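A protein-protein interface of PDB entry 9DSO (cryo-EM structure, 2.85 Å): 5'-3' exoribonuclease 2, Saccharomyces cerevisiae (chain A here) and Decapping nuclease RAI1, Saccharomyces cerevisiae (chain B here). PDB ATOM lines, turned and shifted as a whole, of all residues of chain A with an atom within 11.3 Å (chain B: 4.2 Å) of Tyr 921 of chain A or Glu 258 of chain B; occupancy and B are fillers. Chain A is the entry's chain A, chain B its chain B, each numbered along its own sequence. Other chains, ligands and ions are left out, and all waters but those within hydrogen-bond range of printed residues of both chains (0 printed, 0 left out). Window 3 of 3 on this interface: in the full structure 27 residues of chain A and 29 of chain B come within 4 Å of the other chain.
Of chain A, only Tyr 921 comes within 4 Å of Glu 258 of chain B. Of the printed residues of chain A, Val 248 of chain B touches Gly 919, Gly 920, Tyr 921 and Phe 924. No residue of chain A comes within 4 Å of Arg 259 of chain B. Of the printed residues of chain A, Asn 305 of chain B touches Tyr 921 (2.6 Å) and Phe 925 (3.3 Å). No residue of chain A comes within 4 Å of Val 309 of chain B. Printed residues of chain B within 4 Å of Phe 924 of chain A: Val 248 (3.9 Å) and Thr 254 (3.6 Å). Of the printed residues of chain A, Phe 280 of chain B touches Gly 919 (3.3 Å) and Tyr 921 (3.8 Å). Lys 915 of chain A touches none of the printed residues of chain B. Glu 929 of chain A touches none of the printed residues of chain B. The nearest residue of chain B that does not touch Tyr 921 of chain A is Leu 301 of chain B (4.1 Å). The nearest printed residue of chain B that does not touch Phe 924 of chain A is Glu 291 of chain B (5.4 Å).
Printed residues of chain A that touch a printed residue of chain B: Gly 919, Gly 920, Tyr 921, Arg 922, Ala 923, Phe 924 and Phe 925. Hydrophobic or aromatic side chains of chain A that line the printed part of chain B: Tyr 921, Ala 923, Phe 924 and Phe 925. Of the 17 printed residues of chain B, 7 touch a printed residue of chain A. Among the printed residues, 17 pairs touch across the chains.
The backbone carbonyl oxygen of Gly 919 of chain A is in hydrogen-bond range of the backbone NH of Val 248 of chain B (3.3 Å). OE2 of Glu 258 of chain B is in hydrogen-bond range of OH of Tyr 921 of chain A (2.6 Å). ND2 of Asn 305 of chain B sits at hydrogen-bond distance from OH of Tyr 921 of chain A (2.6 Å). N of Arg 922 of chain A sits at hydrogen-bond distance from OE1 of Glu 291 of chain B, 2.9 Å away. The side-chain carboxylate (OE2) of Glu 291 of chain B lies within hydrogen-bond range of the backbone NH (N) of Ala 923 of chain A (3.1 Å).
Among the printed residues, pairs that only touch across the chains: Gly 919 of chain A with Phe 280 of chain B (3.3 Å), Gly 920 of chain A with Val 248 of chain B (3.2 Å), Gly 920 of chain A with Glu 291 of chain B (3.8 Å), Tyr 921 of chain A with Val 248 of chain B (3.6 Å), Tyr 921 of chain A with Thr 254 of chain B (3.5 Å), Tyr 921 of chain A with Phe 257 of chain B (3.3 Å), Tyr 921 of chain A with Phe 280 of chain B (3.8 Å), Tyr 921 of chain A with Glu 291 of chain B (3.6 Å), Phe 924 of chain A with Val 248 of chain B (3.9 Å), Phe 924 of chain A with Thr 254 of chain B (3.6 Å), Phe 925 of chain A with Thr 254 of chain B (3.8 Å) and Phe 925 of chain A with Asn 305 of chain B (3.3 Å).
ND1 of His 255 of chain B sits at hydrogen-bond distance from OE1 of Glu 258 of chain B, at 3.1 Å. The side-chain amide nitrogen (ND2) of Asn 306 of chain B sits at hydrogen-bond distance from the side-chain carboxylate (OE1) of Glu 258 of chain B, at 3.1 Å.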
ATOM      1  N   TYR A 914      -0.521 -31.176  -4.782  1.00  0.00           N
ATOM      2  CA  TYR A 914      -0.407 -30.669  -3.424  1.00  0.00           C
ATOM      3  C   TYR A 914      -1.602 -31.130  -2.605  1.00  0.00           C
ATOM      4  O   TYR A 914      -2.750 -30.927  -3.007  1.00  0.00           O
ATOM      5  CB  TYR A 914      -0.322 -29.143  -3.420  1.00  0.00           C
ATOM      6  CG  TYR A 914       0.894 -28.603  -4.126  1.00  0.00           C
ATOM      7  CD1 TYR A 914       2.155 -28.756  -3.580  1.00  0.00           C
ATOM      8  CD2 TYR A 914       0.782 -27.941  -5.333  1.00  0.00           C
ATOM      9  CE1 TYR A 914       3.266 -28.272  -4.213  1.00  0.00           C
ATOM     10  CE2 TYR A 914       1.892 -27.453  -5.974  1.00  0.00           C
ATOM     11  CZ  TYR A 914       3.132 -27.623  -5.409  1.00  0.00           C
ATOM     12  OH  TYR A 914       4.246 -27.135  -6.045  1.00  0.00           O
ATOM     13  N   LYS A 915      -1.331 -31.750  -1.471  1.00  0.00           N
ATOM     14  CA  LYS A 915      -2.400 -32.199  -0.598  1.00  0.00           C
ATOM     15  C   LYS A 915      -2.973 -31.024   0.194  1.00  0.00           C
ATOM     16  O   LYS A 915      -2.284 -30.027   0.418  1.00  0.00           O
ATOM     17  CB  LYS A 915      -1.892 -33.275   0.356  1.00  0.00           C
ATOM     18  CG  LYS A 915      -0.779 -32.821   1.267  1.00  0.00           C
ATOM     19  CD  LYS A 915      -0.305 -33.947   2.161  1.00  0.00           C
ATOM     20  CE  LYS A 915      -1.214 -34.117   3.359  1.00  0.00           C
ATOM     21  NZ  LYS A 915      -1.189 -32.931   4.259  1.00  0.00           N
ATOM     22  N   PRO A 916      -4.240 -31.107   0.601  1.00  0.00           N
ATOM     23  CA  PRO A 916      -4.822 -30.026   1.402  1.00  0.00           C
ATOM     24  C   PRO A 916      -4.074 -29.838   2.711  1.00  0.00           C
ATOM     25  O   PRO A 916      -3.636 -30.800   3.344  1.00  0.00           O
ATOM     26  CB  PRO A 916      -6.260 -30.494   1.637  1.00  0.00           C
ATOM     27  CG  PRO A 916      -6.532 -31.432   0.527  1.00  0.00           C
ATOM     28  CD  PRO A 916      -5.241 -32.126   0.249  1.00  0.00           C
ATOM     29  N   ARG A 917      -3.939 -28.580   3.116  1.00  0.00           N
ATOM     30  CA  ARG A 917      -3.158 -28.226   4.289  1.00  0.00           C
ATOM     31  C   ARG A 917      -3.710 -26.927   4.853  1.00  0.00           C
ATOM     32  O   ARG A 917      -4.010 -26.001   4.099  1.00  0.00           O
ATOM     33  CB  ARG A 917      -1.676 -28.088   3.930  1.00  0.00           C
ATOM     34  CG  ARG A 917      -0.740 -28.085   5.112  1.00  0.00           C
ATOM     35  CD  ARG A 917       0.712 -28.115   4.661  1.00  0.00           C
ATOM     36  NE  ARG A 917       1.128 -29.415   4.151  1.00  0.00           N
ATOM     37  CZ  ARG A 917       1.235 -29.717   2.865  1.00  0.00           C
ATOM     38  NH1 ARG A 917       0.907 -28.853   1.922  1.00  0.00           N
ATOM     39  NH2 ARG A 917       1.690 -30.916   2.516  1.00  0.00           N
ATOM     40  N   THR A 918      -3.829 -26.865   6.177  1.00  0.00           N
ATOM     41  CA  THR A 918      -4.501 -25.748   6.832  1.00  0.00           C
ATOM     42  C   THR A 918      -3.883 -24.419   6.417  1.00  0.00           C
ATOM     43  O   THR A 918      -2.660 -24.263   6.404  1.00  0.00           O
ATOM     44  CB  THR A 918      -4.423 -25.910   8.349  1.00  0.00           C
ATOM     45  OG1 THR A 918      -5.017 -27.157   8.726  1.00  0.00           O
ATOM     46  CG2 THR A 918      -5.155 -24.782   9.044  1.00  0.00           C
ATOM     47  N   GLY A 919      -4.740 -23.460   6.077  1.00  0.00           N
ATOM     48  CA  GLY A 919      -4.304 -22.170   5.593  1.00  0.00           C
ATOM     49  C   GLY A 919      -4.556 -21.912   4.124  1.00  0.00           C
ATOM     50  O   GLY A 919      -4.082 -20.897   3.605  1.00  0.00           O
ATOM     51  N   GLY A 920      -5.276 -22.791   3.438  1.00  0.00           N
ATOM     52  CA  GLY A 920      -5.576 -22.599   2.037  1.00  0.00           C
ATOM     53  C   GLY A 920      -7.061 -22.508   1.773  1.00  0.00           C
ATOM     54  O   GLY A 920      -7.867 -22.947   2.593  1.00  0.00           O
ATOM     55  N   TYR A 921      -7.434 -21.926   0.633  1.00  0.00           N
ATOM     56  CA  TYR A 921      -8.841 -21.751   0.292  1.00  0.00           C
ATOM     57  C   TYR A 921      -9.543 -23.096   0.139  1.00  0.00           C
ATOM     58  O   TYR A 921     -10.464 -23.436   0.899  1.00  0.00           O
ATOM     59  CB  TYR A 921      -8.935 -20.936  -0.995  1.00  0.00           C
ATOM     60  CG  TYR A 921     -10.326 -20.553  -1.429  1.00  0.00           C
ATOM     61  CD1 TYR A 921     -11.104 -19.700  -0.662  1.00  0.00           C
ATOM     62  CD2 TYR A 921     -10.850 -21.020  -2.624  1.00  0.00           C
ATOM     63  CE1 TYR A 921     -12.363 -19.336  -1.066  1.00  0.00           C
ATOM     64  CE2 TYR A 921     -12.110 -20.664  -3.035  1.00  0.00           C
ATOM     65  CZ  TYR A 921     -12.863 -19.823  -2.253  1.00  0.00           C
ATOM     66  OH  TYR A 921     -14.125 -19.467  -2.658  1.00  0.00           O
ATOM     67  N   ARG A 922      -9.108 -23.881  -0.849  1.00  0.00           N
ATOM     68  CA  ARG A 922      -9.658 -25.214  -1.041  1.00  0.00           C
ATOM     69  C   ARG A 922      -9.446 -26.086   0.181  1.00  0.00           C
ATOM     70  O   ARG A 922     -10.307 -26.904   0.510  1.00  0.00           O
ATOM     71  CB  ARG A 922      -9.028 -25.871  -2.260  1.00  0.00           C
ATOM     72  CG  ARG A 922      -9.579 -25.381  -3.562  1.00  0.00           C
ATOM     73  CD  ARG A 922      -8.791 -25.937  -4.713  1.00  0.00           C
ATOM     74  NE  ARG A 922      -9.553 -25.853  -5.947  1.00  0.00           N
ATOM     75  CZ  ARG A 922      -9.043 -26.060  -7.149  1.00  0.00           C
ATOM     76  NH1 ARG A 922      -7.761 -26.333  -7.317  1.00  0.00           N
ATOM     77  NH2 ARG A 922      -9.838 -25.991  -8.209  1.00  0.00           N
ATOM     78  N   ALA A 923      -8.310 -25.934   0.858  1.00  0.00           N
ATOM     79  CA  ALA A 923      -8.095 -26.659   2.101  1.00  0.00           C
ATOM     80  C   ALA A 923      -9.106 -26.247   3.159  1.00  0.00           C
ATOM     81  O   ALA A 923      -9.610 -27.092   3.902  1.00  0.00           O
ATOM     82  CB  ALA A 923      -6.672 -26.434   2.596  1.00  0.00           C
ATOM     83  N   PHE A 924      -9.417 -24.951   3.243  1.00  0.00           N
ATOM     84  CA  PHE A 924     -10.414 -24.494   4.208  1.00  0.00           C
ATOM     85  C   PHE A 924     -11.764 -25.141   3.944  1.00  0.00           C
ATOM     86  O   PHE A 924     -12.413 -25.646   4.869  1.00  0.00           O
ATOM     87  CB  PHE A 924     -10.539 -22.970   4.163  1.00  0.00           C
ATOM     88  CG  PHE A 924     -11.692 -22.428   4.963  1.00  0.00           C
ATOM     89  CD1 PHE A 924     -11.603 -22.308   6.336  1.00  0.00           C
ATOM     90  CD2 PHE A 924     -12.861 -22.032   4.340  1.00  0.00           C
ATOM     91  CE1 PHE A 924     -12.659 -21.811   7.071  1.00  0.00           C
ATOM     92  CE2 PHE A 924     -13.920 -21.539   5.071  1.00  0.00           C
ATOM     93  CZ  PHE A 924     -13.817 -21.427   6.436  1.00  0.00           C
ATOM     94  N   PHE A 925     -12.198 -25.155   2.683  1.00  0.00           N
ATOM     95  CA  PHE A 925     -13.497 -25.750   2.378  1.00  0.00           C
ATOM     96  C   PHE A 925     -13.483 -27.263   2.571  1.00  0.00           C
ATOM     97  O   PHE A 925     -14.456 -27.840   3.074  1.00  0.00           O
ATOM     98  CB  PHE A 925     -13.919 -25.381   0.961  1.00  0.00           C
ATOM     99  CG  PHE A 925     -14.510 -24.013   0.858  1.00  0.00           C
ATOM    100  CD1 PHE A 925     -15.681 -23.705   1.522  1.00  0.00           C
ATOM    101  CD2 PHE A 925     -13.884 -23.027   0.123  1.00  0.00           C
ATOM    102  CE1 PHE A 925     -16.225 -22.446   1.441  1.00  0.00           C
ATOM    103  CE2 PHE A 925     -14.422 -21.769   0.040  1.00  0.00           C
ATOM    104  CZ  PHE A 925     -15.594 -21.475   0.698  1.00  0.00           C
ATOM    105  N   TYR A 926     -12.384 -27.920   2.191  1.00  0.00           N
ATOM    106  CA  TYR A 926     -12.271 -29.363   2.369  1.00  0.00           C
ATOM    107  C   TYR A 926     -12.324 -29.744   3.841  1.00  0.00           C
ATOM    108  O   TYR A 926     -13.008 -30.701   4.212  1.00  0.00           O
ATOM    109  CB  TYR A 926     -10.978 -29.861   1.725  1.00  0.00           C
ATOM    110  CG  TYR A 926     -10.551 -31.246   2.151  1.00  0.00           C
ATOM    111  CD1 TYR A 926     -11.277 -32.367   1.770  1.00  0.00           C
ATOM    112  CD2 TYR A 926      -9.416 -31.437   2.923  1.00  0.00           C
ATOM    113  CE1 TYR A 926     -10.888 -33.632   2.152  1.00  0.00           C
ATOM    114  CE2 TYR A 926      -9.021 -32.698   3.309  1.00  0.00           C
ATOM    115  CZ  TYR A 926      -9.759 -33.791   2.921  1.00  0.00           C
ATOM    116  OH  TYR A 926      -9.364 -35.050   3.304  1.00  0.00           O
ATOM    117  N   PHE A 927     -11.626 -28.998   4.698  1.00  0.00           N
ATOM    118  CA  PHE A 927     -11.633 -29.314   6.121  1.00  0.00           C
ATOM    119  C   PHE A 927     -12.959 -28.951   6.773  1.00  0.00           C
ATOM    120  O   PHE A 927     -13.392 -29.636   7.706  1.00  0.00           O
ATOM    121  CB  PHE A 927     -10.472 -28.609   6.817  1.00  0.00           C
ATOM    122  CG  PHE A 927      -9.132 -29.194   6.483  1.00  0.00           C
ATOM    123  CD1 PHE A 927      -8.950 -30.563   6.451  1.00  0.00           C
ATOM    124  CD2 PHE A 927      -8.060 -28.375   6.176  1.00  0.00           C
ATOM    125  CE1 PHE A 927      -7.724 -31.103   6.136  1.00  0.00           C
ATOM    126  CE2 PHE A 927      -6.834 -28.912   5.855  1.00  0.00           C
ATOM    127  CZ  PHE A 927      -6.665 -30.276   5.837  1.00  0.00           C
ATOM    128  N   ALA A 928     -13.629 -27.895   6.300  1.00  0.00           N
ATOM    129  CA  ALA A 928     -14.969 -27.609   6.798  1.00  0.00           C
ATOM    130  C   ALA A 928     -15.928 -28.746   6.468  1.00  0.00           C
ATOM    131  O   ALA A 928     -16.692 -29.196   7.331  1.00  0.00           O
ATOM    132  CB  ALA A 928     -15.479 -26.291   6.217  1.00  0.00           C
ATOM    133  N   GLU A 929     -15.890 -29.236   5.226  1.00  0.00           N
ATOM    134  CA  GLU A 929     -16.737 -30.364   4.853  1.00  0.00           C
ATOM    135  C   GLU A 929     -16.355 -31.622   5.622  1.00  0.00           C
ATOM    136  O   GLU A 929     -17.226 -32.414   5.996  1.00  0.00           O
ATOM    137  CB  GLU A 929     -16.657 -30.607   3.346  1.00  0.00           C
ATOM    138  CG  GLU A 929     -16.828 -32.062   2.931  1.00  0.00           C
ATOM    139  CD  GLU A 929     -18.264 -32.541   3.037  1.00  0.00           C
ATOM    140  OE1 GLU A 929     -19.161 -31.703   3.273  1.00  0.00           O
ATOM    141  OE2 GLU A 929     -18.498 -33.757   2.884  1.00  0.00           O
ATOM    142  N   LEU A 930     -15.059 -31.824   5.862  1.00  0.00           N
ATOM    143  CA  LEU A 930     -14.615 -32.987   6.623  1.00  0.00           C
ATOM    144  C   LEU A 930     -15.143 -32.945   8.050  1.00  0.00           C
ATOM    145  O   LEU A 930     -15.602 -33.964   8.580  1.00  0.00           O
ATOM    146  CB  LEU A 930     -13.089 -33.053   6.612  1.00  0.00           C
ATOM    147  CG  LEU A 930     -12.421 -34.329   7.109  1.00  0.00           C
ATOM    148  CD1 LEU A 930     -12.620 -35.448   6.102  1.00  0.00           C
ATOM    149  CD2 LEU A 930     -10.947 -34.084   7.359  1.00  0.00           C
ATOM    150  N   VAL B 248      -5.834 -18.181   4.457  1.00  0.00           N
ATOM    151  CA  VAL B 248      -7.234 -17.988   4.818  1.00  0.00           C
ATOM    152  C   VAL B 248      -7.523 -18.788   6.080  1.00  0.00           C
ATOM    153  O   VAL B 248      -7.045 -19.915   6.247  1.00  0.00           O
ATOM    154  CB  VAL B 248      -8.173 -18.385   3.660  1.00  0.00           C
ATOM    155  CG1 VAL B 248      -7.775 -17.677   2.378  1.00  0.00           C
ATOM    156  CG2 VAL B 248      -8.204 -19.869   3.458  1.00  0.00           C
ATOM    157  N   THR B 254     -11.968 -15.815   3.334  1.00  0.00           N
ATOM    158  CA  THR B 254     -12.477 -16.514   2.160  1.00  0.00           C
ATOM    159  C   THR B 254     -12.971 -15.531   1.105  1.00  0.00           C
ATOM    160  O   THR B 254     -12.617 -15.647  -0.074  1.00  0.00           O
ATOM    161  CB  THR B 254     -13.596 -17.470   2.576  1.00  0.00           C
ATOM    162  OG1 THR B 254     -13.035 -18.610   3.236  1.00  0.00           O
ATOM    163  CG2 THR B 254     -14.413 -17.917   1.382  1.00  0.00           C
ATOM    164  N   HIS B 255     -13.767 -14.540   1.511  1.00  0.00           N
ATOM    165  CA  HIS B 255     -14.270 -13.559   0.549  1.00  0.00           C
ATOM    166  C   HIS B 255     -13.152 -12.677   0.002  1.00  0.00           C
ATOM    167  O   HIS B 255     -13.129 -12.361  -1.198  1.00  0.00           O
ATOM    168  CB  HIS B 255     -15.360 -12.708   1.196  1.00  0.00           C
ATOM    169  CG  HIS B 255     -16.552 -13.496   1.636  1.00  0.00           C
ATOM    170  ND1 HIS B 255     -16.930 -14.673   1.028  1.00  0.00           N
ATOM    171  CD2 HIS B 255     -17.447 -13.283   2.630  1.00  0.00           C
ATOM    172  CE1 HIS B 255     -18.008 -15.150   1.624  1.00  0.00           C
ATOM    173  NE2 HIS B 255     -18.341 -14.325   2.600  1.00  0.00           N
ATOM    174  N   LYS B 256     -12.223 -12.257   0.866  1.00  0.00           N
ATOM    175  CA  LYS B 256     -11.085 -11.474   0.391  1.00  0.00           C
ATOM    176  C   LYS B 256     -10.306 -12.239  -0.670  1.00  0.00           C
ATOM    177  O   LYS B 256      -9.956 -11.692  -1.730  1.00  0.00           O
ATOM    178  CB  LYS B 256     -10.169 -11.119   1.560  1.00  0.00           C
ATOM    179  CG  LYS B 256     -10.777 -10.193   2.594  1.00  0.00           C
ATOM    180  CD  LYS B 256      -9.812  -9.985   3.748  1.00  0.00           C
ATOM    181  CE  LYS B 256     -10.278  -8.881   4.679  1.00  0.00           C
ATOM    182  NZ  LYS B 256     -11.490  -9.269   5.446  1.00  0.00           N
ATOM    183  N   PHE B 257     -10.043 -13.519  -0.407  1.00  0.00           N
ATOM    184  CA  PHE B 257      -9.343 -14.336  -1.380  1.00  0.00           C
ATOM    185  C   PHE B 257     -10.167 -14.522  -2.640  1.00  0.00           C
ATOM    186  O   PHE B 257      -9.610 -14.678  -3.725  1.00  0.00           O
ATOM    187  CB  PHE B 257      -8.994 -15.694  -0.790  1.00  0.00           C
ATOM    188  CG  PHE B 257      -8.449 -16.639  -1.801  1.00  0.00           C
ATOM    189  CD1 PHE B 257      -7.138 -16.551  -2.196  1.00  0.00           C
ATOM    190  CD2 PHE B 257      -9.260 -17.579  -2.399  1.00  0.00           C
ATOM    191  CE1 PHE B 257      -6.645 -17.400  -3.130  1.00  0.00           C
ATOM    192  CE2 PHE B 257      -8.762 -18.428  -3.345  1.00  0.00           C
ATOM    193  CZ  PHE B 257      -7.457 -18.343  -3.705  1.00  0.00           C
ATOM    194  N   GLU B 258     -11.494 -14.551  -2.518  1.00  0.00           N
ATOM    195  CA  GLU B 258     -12.318 -14.677  -3.714  1.00  0.00           C
ATOM    196  C   GLU B 258     -12.170 -13.462  -4.620  1.00  0.00           C
ATOM    197  O   GLU B 258     -12.076 -13.604  -5.843  1.00  0.00           O
ATOM    198  CB  GLU B 258     -13.776 -14.905  -3.331  1.00  0.00           C
ATOM    199  CG  GLU B 258     -14.059 -16.336  -2.933  1.00  0.00           C
ATOM    200  CD  GLU B 258     -15.321 -16.483  -2.126  1.00  0.00           C
ATOM    201  OE1 GLU B 258     -15.938 -15.451  -1.799  1.00  0.00           O
ATOM    202  OE2 GLU B 258     -15.689 -17.629  -1.805  1.00  0.00           O
ATOM    203  N   ARG B 259     -12.139 -12.258  -4.044  1.00  0.00           N
ATOM    204  CA  ARG B 259     -11.877 -11.078  -4.875  1.00  0.00           C
ATOM    205  C   ARG B 259     -10.488 -11.130  -5.510  1.00  0.00           C
ATOM    206  O   ARG B 259     -10.325 -10.823  -6.704  1.00  0.00           O
ATOM    207  CB  ARG B 259     -12.051  -9.782  -4.081  1.00  0.00           C
ATOM    208  CG  ARG B 259     -13.494  -9.316  -3.908  1.00  0.00           C
ATOM    209  CD  ARG B 259     -14.217  -9.971  -2.755  1.00  0.00           C
ATOM    210  NE  ARG B 259     -13.554  -9.729  -1.478  1.00  0.00           N
ATOM    211  CZ  ARG B 259     -13.733  -8.643  -0.737  1.00  0.00           C
ATOM    212  NH1 ARG B 259     -14.533  -7.665  -1.128  1.00  0.00           N
ATOM    213  NH2 ARG B 259     -13.094  -8.536   0.424  1.00  0.00           N
ATOM    214  N   LYS B 260      -9.471 -11.521  -4.736  1.00  0.00           N
ATOM    215  CA  LYS B 260      -8.130 -11.623  -5.313  1.00  0.00           C
ATOM    216  C   LYS B 260      -8.074 -12.674  -6.421  1.00  0.00           C
ATOM    217  O   LYS B 260      -7.415 -12.472  -7.452  1.00  0.00           O
ATOM    218  CB  LYS B 260      -7.107 -11.936  -4.224  1.00  0.00           C
ATOM    219  CG  LYS B 260      -6.741 -10.742  -3.365  1.00  0.00           C
ATOM    220  CD  LYS B 260      -5.597 -11.064  -2.427  1.00  0.00           C
ATOM    221  CE  LYS B 260      -6.071 -11.863  -1.235  1.00  0.00           C
ATOM    222  NZ  LYS B 260      -5.000 -12.017  -0.217  1.00  0.00           N
ATOM    223  N   LEU B 261      -8.762 -13.798  -6.223  1.00  0.00           N
ATOM    224  CA  LEU B 261      -8.796 -14.860  -7.219  1.00  0.00           C
ATOM    225  C   LEU B 261      -9.532 -14.413  -8.470  1.00  0.00           C
ATOM    226  O   LEU B 261      -9.173 -14.812  -9.581  1.00  0.00           O
ATOM    227  CB  LEU B 261      -9.452 -16.105  -6.626  1.00  0.00           C
ATOM    228  CG  LEU B 261      -9.628 -17.340  -7.513  1.00  0.00           C
ATOM    229  CD1 LEU B 261      -8.307 -17.786  -8.105  1.00  0.00           C
ATOM    230  CD2 LEU B 261     -10.286 -18.469  -6.740  1.00  0.00           C
ATOM    231  N   PHE B 262     -10.572 -13.593  -8.315  1.00  0.00           N
ATOM    232  CA  PHE B 262     -11.237 -13.029  -9.484  1.00  0.00           C
ATOM    233  C   PHE B 262     -10.283 -12.156 -10.286  1.00  0.00           C
ATOM    234  O   PHE B 262     -10.237 -12.238 -11.520  1.00  0.00           O
ATOM    235  CB  PHE B 262     -12.462 -12.220  -9.063  1.00  0.00           C
ATOM    236  CG  PHE B 262     -13.089 -11.453 -10.190  1.00  0.00           C
ATOM    237  CD1 PHE B 262     -13.928 -12.083 -11.085  1.00  0.00           C
ATOM    238  CD2 PHE B 262     -12.822 -10.108 -10.369  1.00  0.00           C
ATOM    239  CE1 PHE B 262     -14.493 -11.386 -12.124  1.00  0.00           C
ATOM    240  CE2 PHE B 262     -13.385  -9.410 -11.412  1.00  0.00           C
ATOM    241  CZ  PHE B 262     -14.221 -10.048 -12.289  1.00  0.00           C
ATOM    242  N   PHE B 280       0.090 -19.607  -0.014  1.00  0.00           N
ATOM    243  CA  PHE B 280      -0.536 -19.016   1.158  1.00  0.00           C
ATOM    244  C   PHE B 280       0.489 -18.977   2.279  1.00  0.00           C
ATOM    245  O   PHE B 280       1.016 -20.026   2.678  1.00  0.00           O
ATOM    246  CB  PHE B 280      -1.765 -19.810   1.588  1.00  0.00           C
ATOM    247  CG  PHE B 280      -2.867 -19.819   0.574  1.00  0.00           C
ATOM    248  CD1 PHE B 280      -2.890 -20.767  -0.430  1.00  0.00           C
ATOM    249  CD2 PHE B 280      -3.881 -18.887   0.629  1.00  0.00           C
ATOM    250  CE1 PHE B 280      -3.895 -20.778  -1.361  1.00  0.00           C
ATOM    251  CE2 PHE B 280      -4.889 -18.898  -0.299  1.00  0.00           C
ATOM    252  CZ  PHE B 280      -4.896 -19.846  -1.296  1.00  0.00           C
ATOM    253  N   GLU B 291      -1.629 -23.993  -3.493  1.00  0.00           N
ATOM    254  CA  GLU B 291      -2.832 -24.525  -4.121  1.00  0.00           C
ATOM    255  C   GLU B 291      -2.840 -24.190  -5.604  1.00  0.00           C
ATOM    256  O   GLU B 291      -2.353 -23.136  -6.013  1.00  0.00           O
ATOM    257  CB  GLU B 291      -4.089 -23.976  -3.460  1.00  0.00           C
ATOM    258  CG  GLU B 291      -4.129 -24.211  -1.971  1.00  0.00           C
ATOM    259  CD  GLU B 291      -5.500 -24.593  -1.489  1.00  0.00           C
ATOM    260  OE1 GLU B 291      -6.481 -24.113  -2.087  1.00  0.00           O
ATOM    261  OE2 GLU B 291      -5.596 -25.373  -0.519  1.00  0.00           O
ATOM    262  N   LEU B 301     -16.185 -22.044  -9.723  1.00  0.00           N
ATOM    263  CA  LEU B 301     -15.862 -22.089  -8.301  1.00  0.00           C
ATOM    264  C   LEU B 301     -16.338 -20.831  -7.587  1.00  0.00           C
ATOM    265  O   LEU B 301     -16.903 -20.902  -6.489  1.00  0.00           O
ATOM    266  CB  LEU B 301     -14.355 -22.263  -8.131  1.00  0.00           C
ATOM    267  CG  LEU B 301     -13.760 -22.383  -6.733  1.00  0.00           C
ATOM    268  CD1 LEU B 301     -14.174 -23.691  -6.094  1.00  0.00           C
ATOM    269  CD2 LEU B 301     -12.252 -22.283  -6.825  1.00  0.00           C
ATOM    270  N   LEU B 302     -16.118 -19.667  -8.201  1.00  0.00           N
ATOM    271  CA  LEU B 302     -16.575 -18.413  -7.617  1.00  0.00           C
ATOM    272  C   LEU B 302     -18.093 -18.373  -7.526  1.00  0.00           C
ATOM    273  O   LEU B 302     -18.644 -17.910  -6.524  1.00  0.00           O
ATOM    274  CB  LEU B 302     -16.050 -17.235  -8.436  1.00  0.00           C
ATOM    275  CG  LEU B 302     -14.546 -16.969  -8.347  1.00  0.00           C
ATOM    276  CD1 LEU B 302     -14.115 -15.936  -9.369  1.00  0.00           C
ATOM    277  CD2 LEU B 302     -14.159 -16.529  -6.951  1.00  0.00           C
ATOM    278  N   ASN B 305     -19.173 -20.546  -4.654  1.00  0.00           N
ATOM    279  CA  ASN B 305     -18.767 -20.057  -3.343  1.00  0.00           C
ATOM    280  C   ASN B 305     -19.259 -18.648  -3.046  1.00  0.00           C
ATOM    281  O   ASN B 305     -19.593 -18.347  -1.897  1.00  0.00           O
ATOM    282  CB  ASN B 305     -17.243 -20.106  -3.217  1.00  0.00           C
ATOM    283  CG  ASN B 305     -16.715 -21.522  -3.110  1.00  0.00           C
ATOM    284  OD1 ASN B 305     -17.483 -22.475  -2.997  1.00  0.00           O
ATOM    285  ND2 ASN B 305     -15.399 -21.667  -3.149  1.00  0.00           N
ATOM    286  N   ASN B 306     -19.315 -17.777  -4.049  1.00  0.00           N
ATOM    287  CA  ASN B 306     -19.776 -16.401  -3.862  1.00  0.00           C
ATOM    288  C   ASN B 306     -20.383 -15.925  -5.173  1.00  0.00           C
ATOM    289  O   ASN B 306     -19.666 -15.441  -6.062  1.00  0.00           O
ATOM    290  CB  ASN B 306     -18.642 -15.482  -3.420  1.00  0.00           C
ATOM    291  CG  ASN B 306     -19.133 -14.290  -2.623  1.00  0.00           C
ATOM    292  OD1 ASN B 306     -20.324 -14.168  -2.335  1.00  0.00           O
ATOM    293  ND2 ASN B 306     -18.215 -13.403  -2.263  1.00  0.00           N
ATOM    294  N   VAL B 309     -19.421 -12.426  -6.741  1.00  0.00           N
ATOM    295  CA  VAL B 309     -18.172 -12.377  -7.491  1.00  0.00           C
ATOM    296  C   VAL B 309     -18.224 -13.314  -8.693  1.00  0.00           C
ATOM    297  O   VAL B 309     -17.523 -13.094  -9.686  1.00  0.00           O
ATOM    298  CB  VAL B 309     -16.985 -12.713  -6.570  1.00  0.00           C
ATOM    299  CG1 VAL B 309     -15.671 -12.378  -7.243  1.00  0.00           C
ATOM    300  CG2 VAL B 309     -17.114 -11.973  -5.250  1.00  0.00           C
